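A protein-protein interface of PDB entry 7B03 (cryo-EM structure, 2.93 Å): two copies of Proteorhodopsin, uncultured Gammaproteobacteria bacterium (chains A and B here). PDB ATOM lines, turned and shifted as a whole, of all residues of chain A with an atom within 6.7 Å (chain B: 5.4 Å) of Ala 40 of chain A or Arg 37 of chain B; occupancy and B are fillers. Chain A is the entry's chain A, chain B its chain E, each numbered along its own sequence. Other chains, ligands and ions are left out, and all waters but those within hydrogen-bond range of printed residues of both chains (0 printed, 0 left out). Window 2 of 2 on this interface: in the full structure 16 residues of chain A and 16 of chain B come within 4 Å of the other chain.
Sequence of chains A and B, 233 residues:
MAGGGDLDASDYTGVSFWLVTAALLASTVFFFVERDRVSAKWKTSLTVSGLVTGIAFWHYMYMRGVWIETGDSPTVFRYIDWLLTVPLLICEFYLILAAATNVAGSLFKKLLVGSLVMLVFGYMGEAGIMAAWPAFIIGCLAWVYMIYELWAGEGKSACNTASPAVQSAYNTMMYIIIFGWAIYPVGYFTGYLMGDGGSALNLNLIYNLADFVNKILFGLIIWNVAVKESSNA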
ATOM      1  N   ARG A  35      14.248  22.078 -15.915  1.00  0.00           N
ATOM      2  CA  ARG A  35      14.279  20.964 -14.976  1.00  0.00           C
ATOM      3  C   ARG A  35      13.234  21.091 -13.880  1.00  0.00           C
ATOM      4  O   ARG A  35      12.988  20.113 -13.169  1.00  0.00           O
ATOM      5  CB  ARG A  35      15.669  20.837 -14.351  1.00  0.00           C
ATOM      6  CG  ARG A  35      16.736  20.349 -15.310  1.00  0.00           C
ATOM      7  CD  ARG A  35      18.127  20.457 -14.714  1.00  0.00           C
ATOM      8  NE  ARG A  35      18.427  19.387 -13.767  1.00  0.00           N
ATOM      9  CZ  ARG A  35      18.319  19.497 -12.448  1.00  0.00           C
ATOM     10  NH1 ARG A  35      17.916  20.635 -11.904  1.00  0.00           N
ATOM     11  NH2 ARG A  35      18.625  18.470 -11.670  1.00  0.00           N
ATOM     12  N   VAL A  38       9.951  18.877 -14.461  1.00  0.00           N
ATOM     13  CA  VAL A  38      10.093  17.432 -14.463  1.00  0.00           C
ATOM     14  C   VAL A  38      10.270  16.941 -13.032  1.00  0.00           C
ATOM     15  O   VAL A  38      10.649  17.688 -12.125  1.00  0.00           O
ATOM     16  CB  VAL A  38      11.261  16.965 -15.355  1.00  0.00           C
ATOM     17  CG1 VAL A  38      11.119  17.540 -16.745  1.00  0.00           C
ATOM     18  CG2 VAL A  38      12.585  17.367 -14.753  1.00  0.00           C
ATOM     19  N   SER A  39       9.971  15.662 -12.835  1.00  0.00           N
ATOM     20  CA  SER A  39      10.175  15.023 -11.548  1.00  0.00           C
ATOM     21  C   SER A  39      11.668  14.867 -11.268  1.00  0.00           C
ATOM     22  O   SER A  39      12.521  15.155 -12.110  1.00  0.00           O
ATOM     23  CB  SER A  39       9.479  13.666 -11.510  1.00  0.00           C
ATOM     24  OG  SER A  39       9.759  12.989 -10.302  1.00  0.00           O
ATOM     25  N   ALA A  40      11.982  14.407 -10.058  1.00  0.00           N
ATOM     26  CA  ALA A  40      13.381  14.250  -9.677  1.00  0.00           C
ATOM     27  C   ALA A  40      14.089  13.225 -10.552  1.00  0.00           C
ATOM     28  O   ALA A  40      15.280  13.376 -10.843  1.00  0.00           O
ATOM     29  CB  ALA A  40      13.485  13.856  -8.204  1.00  0.00           C
ATOM     30  N   LYS A  41      13.377  12.186 -10.985  1.00  0.00           N
ATOM     31  CA  LYS A  41      14.001  11.139 -11.786  1.00  0.00           C
ATOM     32  C   LYS A  41      14.462  11.662 -13.144  1.00  0.00           C
ATOM     33  O   LYS A  41      15.533  11.278 -13.627  1.00  0.00           O
ATOM     34  CB  LYS A  41      13.032   9.972 -11.943  1.00  0.00           C
ATOM     35  CG  LYS A  41      11.594  10.397 -12.128  1.00  0.00           C
ATOM     36  CD  LYS A  41      10.629   9.348 -11.610  1.00  0.00           C
ATOM     37  CE  LYS A  41      10.870   8.005 -12.259  1.00  0.00           C
ATOM     38  NZ  LYS A  41       9.852   6.996 -11.863  1.00  0.00           N
ATOM     39  N   TRP A  42      13.677  12.537 -13.774  1.00  0.00           N
ATOM     40  CA  TRP A  42      13.994  13.039 -15.107  1.00  0.00           C
ATOM     41  C   TRP A  42      14.972  14.206 -15.097  1.00  0.00           C
ATOM     42  O   TRP A  42      15.430  14.633 -16.171  1.00  0.00           O
ATOM     43  CB  TRP A  42      12.709  13.457 -15.811  1.00  0.00           C
ATOM     44  CG  TRP A  42      11.709  12.363 -15.906  1.00  0.00           C
ATOM     45  CD1 TRP A  42      10.733  12.073 -15.009  1.00  0.00           C
ATOM     46  CD2 TRP A  42      11.581  11.411 -16.963  1.00  0.00           C
ATOM     47  NE1 TRP A  42      10.004  10.995 -15.436  1.00  0.00           N
ATOM     48  CE2 TRP A  42      10.506  10.570 -16.637  1.00  0.00           C
ATOM     49  CE3 TRP A  42      12.275  11.187 -18.153  1.00  0.00           C
ATOM     50  CZ2 TRP A  42      10.106   9.524 -17.454  1.00  0.00           C
ATOM     51  CZ3 TRP A  42      11.877  10.149 -18.964  1.00  0.00           C
ATOM     52  CH2 TRP A  42      10.804   9.331 -18.613  1.00  0.00           C
ATOM     53  N   LYS A  43      15.298  14.728 -13.915  1.00  0.00           N
ATOM     54  CA  LYS A  43      16.192  15.873 -13.832  1.00  0.00           C
ATOM     55  C   LYS A  43      17.585  15.521 -14.328  1.00  0.00           C
ATOM     56  O   LYS A  43      18.255  16.350 -14.948  1.00  0.00           O
ATOM     57  CB  LYS A  43      16.238  16.394 -12.398  1.00  0.00           C
ATOM     58  CG  LYS A  43      15.040  17.242 -12.014  1.00  0.00           C
ATOM     59  CD  LYS A  43      15.192  17.814 -10.619  1.00  0.00           C
ATOM     60  CE  LYS A  43      14.220  18.952 -10.382  1.00  0.00           C
ATOM     61  NZ  LYS A  43      12.814  18.539 -10.618  1.00  0.00           N
ATOM     62  N   THR A  44      18.039  14.295 -14.067  1.00  0.00           N
ATOM     63  CA  THR A  44      19.355  13.890 -14.545  1.00  0.00           C
ATOM     64  C   THR A  44      19.399  13.837 -16.068  1.00  0.00           C
ATOM     65  O   THR A  44      20.398  14.232 -16.680  1.00  0.00           O
ATOM     66  CB  THR A  44      19.744  12.543 -13.934  1.00  0.00           C
ATOM     67  OG1 THR A  44      20.985  12.097 -14.493  1.00  0.00           O
ATOM     68  CG2 THR A  44      18.667  11.501 -14.189  1.00  0.00           C
ATOM     69  N   SER A  45      18.323  13.362 -16.697  1.00  0.00           N
ATOM     70  CA  SER A  45      18.268  13.328 -18.153  1.00  0.00           C
ATOM     71  C   SER A  45      18.329  14.734 -18.732  1.00  0.00           C
ATOM     72  O   SER A  45      19.083  15.002 -19.679  1.00  0.00           O
ATOM     73  CB  SER A  45      16.996  12.619 -18.603  1.00  0.00           C
ATOM     74  OG  SER A  45      17.020  11.260 -18.213  1.00  0.00           O
ATOM     75  N   LEU A  95      19.450   6.689 -19.260  1.00  0.00           N
ATOM     76  CA  LEU A  95      18.823   7.627 -18.335  1.00  0.00           C
ATOM     77  C   LEU A  95      17.304   7.575 -18.434  1.00  0.00           C
ATOM     78  O   LEU A  95      16.608   7.452 -17.419  1.00  0.00           O
ATOM     79  CB  LEU A  95      19.326   9.043 -18.602  1.00  0.00           C
ATOM     80  CG  LEU A  95      20.765   9.335 -18.194  1.00  0.00           C
ATOM     81  CD1 LEU A  95      21.101  10.756 -18.552  1.00  0.00           C
ATOM     82  CD2 LEU A  95      20.959   9.099 -16.709  1.00  0.00           C
ATOM     83  N   SER A 230       5.982  13.713 -15.977  1.00  0.00           N
ATOM     84  CA  SER A 230       5.836  14.408 -14.705  1.00  0.00           C
ATOM     85  C   SER A 230       4.437  14.987 -14.544  1.00  0.00           C
ATOM     86  O   SER A 230       3.855  14.920 -13.457  1.00  0.00           O
ATOM     87  CB  SER A 230       6.892  15.502 -14.588  1.00  0.00           C
ATOM     88  OG  SER A 230       8.182  14.970 -14.813  1.00  0.00           O
ATOM     89  N   GLU B  34      22.719  18.920  -9.971  1.00  0.00           N
ATOM     90  CA  GLU B  34      22.115  17.687  -9.489  1.00  0.00           C
ATOM     91  C   GLU B  34      21.889  17.670  -7.984  1.00  0.00           C
ATOM     92  O   GLU B  34      21.523  16.622  -7.447  1.00  0.00           O
ATOM     93  CB  GLU B  34      22.983  16.494  -9.894  1.00  0.00           C
ATOM     94  CG  GLU B  34      22.841  16.085 -11.349  1.00  0.00           C
ATOM     95  CD  GLU B  34      21.485  15.483 -11.658  1.00  0.00           C
ATOM     96  OE1 GLU B  34      20.527  16.244 -11.893  1.00  0.00           O
ATOM     97  OE2 GLU B  34      21.374  14.242 -11.658  1.00  0.00           O
ATOM     98  N   ARG B  35      22.098  18.788  -7.290  1.00  0.00           N
ATOM     99  CA  ARG B  35      21.799  18.836  -5.864  1.00  0.00           C
ATOM    100  C   ARG B  35      20.310  18.743  -5.572  1.00  0.00           C
ATOM    101  O   ARG B  35      19.938  18.528  -4.416  1.00  0.00           O
ATOM    102  CB  ARG B  35      22.365  20.117  -5.249  1.00  0.00           C
ATOM    103  CG  ARG B  35      23.877  20.144  -5.160  1.00  0.00           C
ATOM    104  CD  ARG B  35      24.398  21.512  -4.760  1.00  0.00           C
ATOM    105  NE  ARG B  35      24.266  21.777  -3.330  1.00  0.00           N
ATOM    106  CZ  ARG B  35      23.273  22.468  -2.781  1.00  0.00           C
ATOM    107  NH1 ARG B  35      22.312  22.973  -3.540  1.00  0.00           N
ATOM    108  NH2 ARG B  35      23.247  22.663  -1.472  1.00  0.00           N
ATOM    109  N   ASP B  36      19.479  18.863  -6.603  1.00  0.00           N
ATOM    110  CA  ASP B  36      18.032  18.791  -6.437  1.00  0.00           C
ATOM    111  C   ASP B  36      17.529  17.369  -6.184  1.00  0.00           C
ATOM    112  O   ASP B  36      16.511  17.176  -5.521  1.00  0.00           O
ATOM    113  CB  ASP B  36      17.327  19.387  -7.657  1.00  0.00           C
ATOM    114  CG  ASP B  36      17.715  20.831  -7.909  1.00  0.00           C
ATOM    115  OD1 ASP B  36      18.570  21.357  -7.163  1.00  0.00           O
ATOM    116  OD2 ASP B  36      17.171  21.441  -8.852  1.00  0.00           O
ATOM    117  N   ARG B  37      18.241  16.379  -6.714  1.00  0.00           N
ATOM    118  CA  ARG B  37      17.844  14.989  -6.544  1.00  0.00           C
ATOM    119  C   ARG B  37      18.257  14.408  -5.203  1.00  0.00           C
ATOM    120  O   ARG B  37      17.826  13.301  -4.873  1.00  0.00           O
ATOM    121  CB  ARG B  37      18.435  14.133  -7.662  1.00  0.00           C
ATOM    122  CG  ARG B  37      17.936  14.469  -9.047  1.00  0.00           C
ATOM    123  CD  ARG B  37      18.248  13.326  -9.985  1.00  0.00           C
ATOM    124  NE  ARG B  37      17.633  12.089  -9.516  1.00  0.00           N
ATOM    125  CZ  ARG B  37      17.892  10.887 -10.018  1.00  0.00           C
ATOM    126  NH1 ARG B  37      17.283   9.820  -9.528  1.00  0.00           N
ATOM    127  NH2 ARG B  37      18.765  10.754 -11.005  1.00  0.00           N
ATOM    128  N   VAL B  38      19.076  15.111  -4.431  1.00  0.00           N
ATOM    129  CA  VAL B  38      19.580  14.582  -3.176  1.00  0.00           C
ATOM    130  C   VAL B  38      18.875  15.275  -2.016  1.00  0.00           C
ATOM    131  O   VAL B  38      18.314  16.368  -2.150  1.00  0.00           O
ATOM    132  CB  VAL B  38      21.110  14.727  -3.057  1.00  0.00           C
ATOM    133  CG1 VAL B  38      21.788  14.118  -4.263  1.00  0.00           C
ATOM    134  CG2 VAL B  38      21.498  16.178  -2.914  1.00  0.00           C
ATOM    135  N   SER B  39      18.896  14.611  -0.866  1.00  0.00           N
ATOM    136  CA  SER B  39      18.348  15.181   0.350  1.00  0.00           C
ATOM    137  C   SER B  39      19.225  16.334   0.833  1.00  0.00           C
ATOM    138  O   SER B  39      20.295  16.611   0.287  1.00  0.00           O
ATOM    139  CB  SER B  39      18.228  14.113   1.433  1.00  0.00           C
ATOM    140  OG  SER B  39      17.795  14.678   2.653  1.00  0.00           O
ATOM    141  N   TRP B 223      27.866  11.287  -6.094  1.00  0.00           N
ATOM    142  CA  TRP B 223      26.547  11.628  -6.614  1.00  0.00           C
ATOM    143  C   TRP B 223      25.658  10.397  -6.720  1.00  0.00           C
ATOM    144  O   TRP B 223      24.468  10.452  -6.393  1.00  0.00           O
ATOM    145  CB  TRP B 223      26.689  12.307  -7.976  1.00  0.00           C
ATOM    146  CG  TRP B 223      25.412  12.428  -8.746  1.00  0.00           C
ATOM    147  CD1 TRP B 223      24.512  13.445  -8.683  1.00  0.00           C
ATOM    148  CD2 TRP B 223      24.898  11.500  -9.708  1.00  0.00           C
ATOM    149  NE1 TRP B 223      23.467  13.208  -9.536  1.00  0.00           N
ATOM    150  CE2 TRP B 223      23.680  12.018 -10.177  1.00  0.00           C
ATOM    151  CE3 TRP B 223      25.347  10.278 -10.209  1.00  0.00           C
ATOM    152  CZ2 TRP B 223      22.911  11.361 -11.122  1.00  0.00           C
ATOM    153  CZ3 TRP B 223      24.580   9.630 -11.146  1.00  0.00           C
ATOM    154  CH2 TRP B 223      23.376  10.171 -11.594  1.00  0.00           C
ATOM    155  N   ALA B 226      24.551   9.393  -3.198  1.00  0.00           N
ATOM    156  CA  ALA B 226      23.620  10.367  -2.640  1.00  0.00           C
ATOM    157  C   ALA B 226      22.248  10.252  -3.284  1.00  0.00           C
ATOM    158  O   ALA B 226      21.224  10.296  -2.592  1.00  0.00           O
ATOM    159  CB  ALA B 226      24.177  11.778  -2.811  1.00  0.00           C
ATOM    160  N   VAL B 227      22.206  10.101  -4.608  1.00  0.00           N
ATOM    161  CA  VAL B 227      20.937   9.955  -5.310  1.00  0.00           C
ATOM    162  C   VAL B 227      20.237   8.675  -4.885  1.00  0.00           C
ATOM    163  O   VAL B 227      19.022   8.663  -4.659  1.00  0.00           O
ATOM    164  CB  VAL B 227      21.165  10.005  -6.830  1.00  0.00           C
ATOM    165  CG1 VAL B 227      19.951   9.487  -7.569  1.00  0.00           C
ATOM    166  CG2 VAL B 227      21.475  11.420  -7.264  1.00  0.00           C
ATOM    167  N   SER B 230      18.828   9.193  -1.327  1.00  0.00           N
ATOM    168  CA  SER B 230      17.676  10.086  -1.307  1.00  0.00           C
ATOM    169  C   SER B 230      16.449   9.424  -1.919  1.00  0.00           C
ATOM    170  O   SER B 230      15.337   9.572  -1.401  1.00  0.00           O
ATOM    171  CB  SER B 230      18.014  11.382  -2.037  1.00  0.00           C
ATOM    172  OG  SER B 230      19.197  11.950  -1.513  1.00  0.00           O
ATOM    173  N   SER B 231      16.627   8.691  -3.020  1.00  0.00           N
ATOM    174  CA  SER B 231      15.488   8.070  -3.685  1.00  0.00           C
ATOM    175  C   SER B 231      14.898   6.946  -2.844  1.00  0.00           C
ATOM    176  O   SER B 231      13.680   6.887  -2.636  1.00  0.00           O
ATOM    177  CB  SER B 231      15.905   7.546  -5.058  1.00  0.00           C
ATOM    178  OG  SER B 231      16.811   6.465  -4.933  1.00  0.00           O
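OE1 of Glu 34 of chain B is in salt-bridge range of NH2 of Arg 35 of chain A.
The guanidinium group (NH1) of Arg 35 of chain A is in salt-bridge range of the side-chain carboxylate (OD2) of Asp 36 of chain B (3.2 Å).
The guanidinium group of Arg 37 of chain B sits at hydrogen-bond distance from the backbone carbonyl oxygen of Ala 40 of chain A (3.0 Å).
The side-chain amino group (NZ) of Lys 43 of chain A lies within hydrogen-bond range of the backbone carbonyl oxygen (O) of Arg 35 of chain A (3.0 Å).
NZ of Lys 43 of chain A is in hydrogen-bond range of O of Val 38 of chain A.
NE1 of Trp 223 of chain B lies within hydrogen-bond range of OE2 of Glu 34 of chain B (3.2 Å).
Lys 43 of chain A touches Glu 34 of chain B (O to OE1, 3.8 Å).
Lys 43 of chain A touches Asp 36 of chain B (CD to CB, 3.98 Å).
Thr 44 of chain A touches Glu 34 of chain B.
CG2 of Thr 44 of chain A touches NH2 of Arg 37 of chain B (3.3 Å).
Thr 44 of chain A touches Trp 223 of chain B (OG1 to CZ2, 3.95 Å).
Printed residues of chain B within 4 Å of Arg 35 of chain A: Glu 34 (2.9 Å) and Asp 36 (3.2 Å).
Of chain B, only Arg 37 (3.0 Å) comes within 4 Å of Ala 40 of chain A.
Of the printed residues of chain B, Thr 44 of chain A touches Glu 34 (3.3 Å), Arg 37 (3.3 Å) and Trp 223 (3.95 Å).
Of the printed residues of chain A, Glu 34 of chain B touches Arg 35 (2.9 Å), Lys 43 (3.8 Å) and Thr 44 (3.3 Å).
Printed residues of chain A within 4 Å of Asp 36 of chain B: Arg 35 and Lys 43.
Of chain A, only Ala 40 (3.0 Å) and Thr 44 (3.3 Å) come within 4 Å of Arg 37 of chain B.
Of the printed residues of chain A, Trp 223 of chain B touches Thr 44 (3.95 Å).
The nearest printed residue of chain A that does not touch Arg 37 of chain B is Lys 41 of chain A (4.2 Å).
The nearest printed residue of chain A that does not touch Trp 223 of chain B is Leu 95 of chain A (5.8 Å).
Of the 11 printed residues of chain A, 4 touch a printed residue of chain B.
4 positions are printed for both chains.
Of the 8 pairs that touch across the chains among the printed residues, none has its exchanged pair printed and touching as well.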
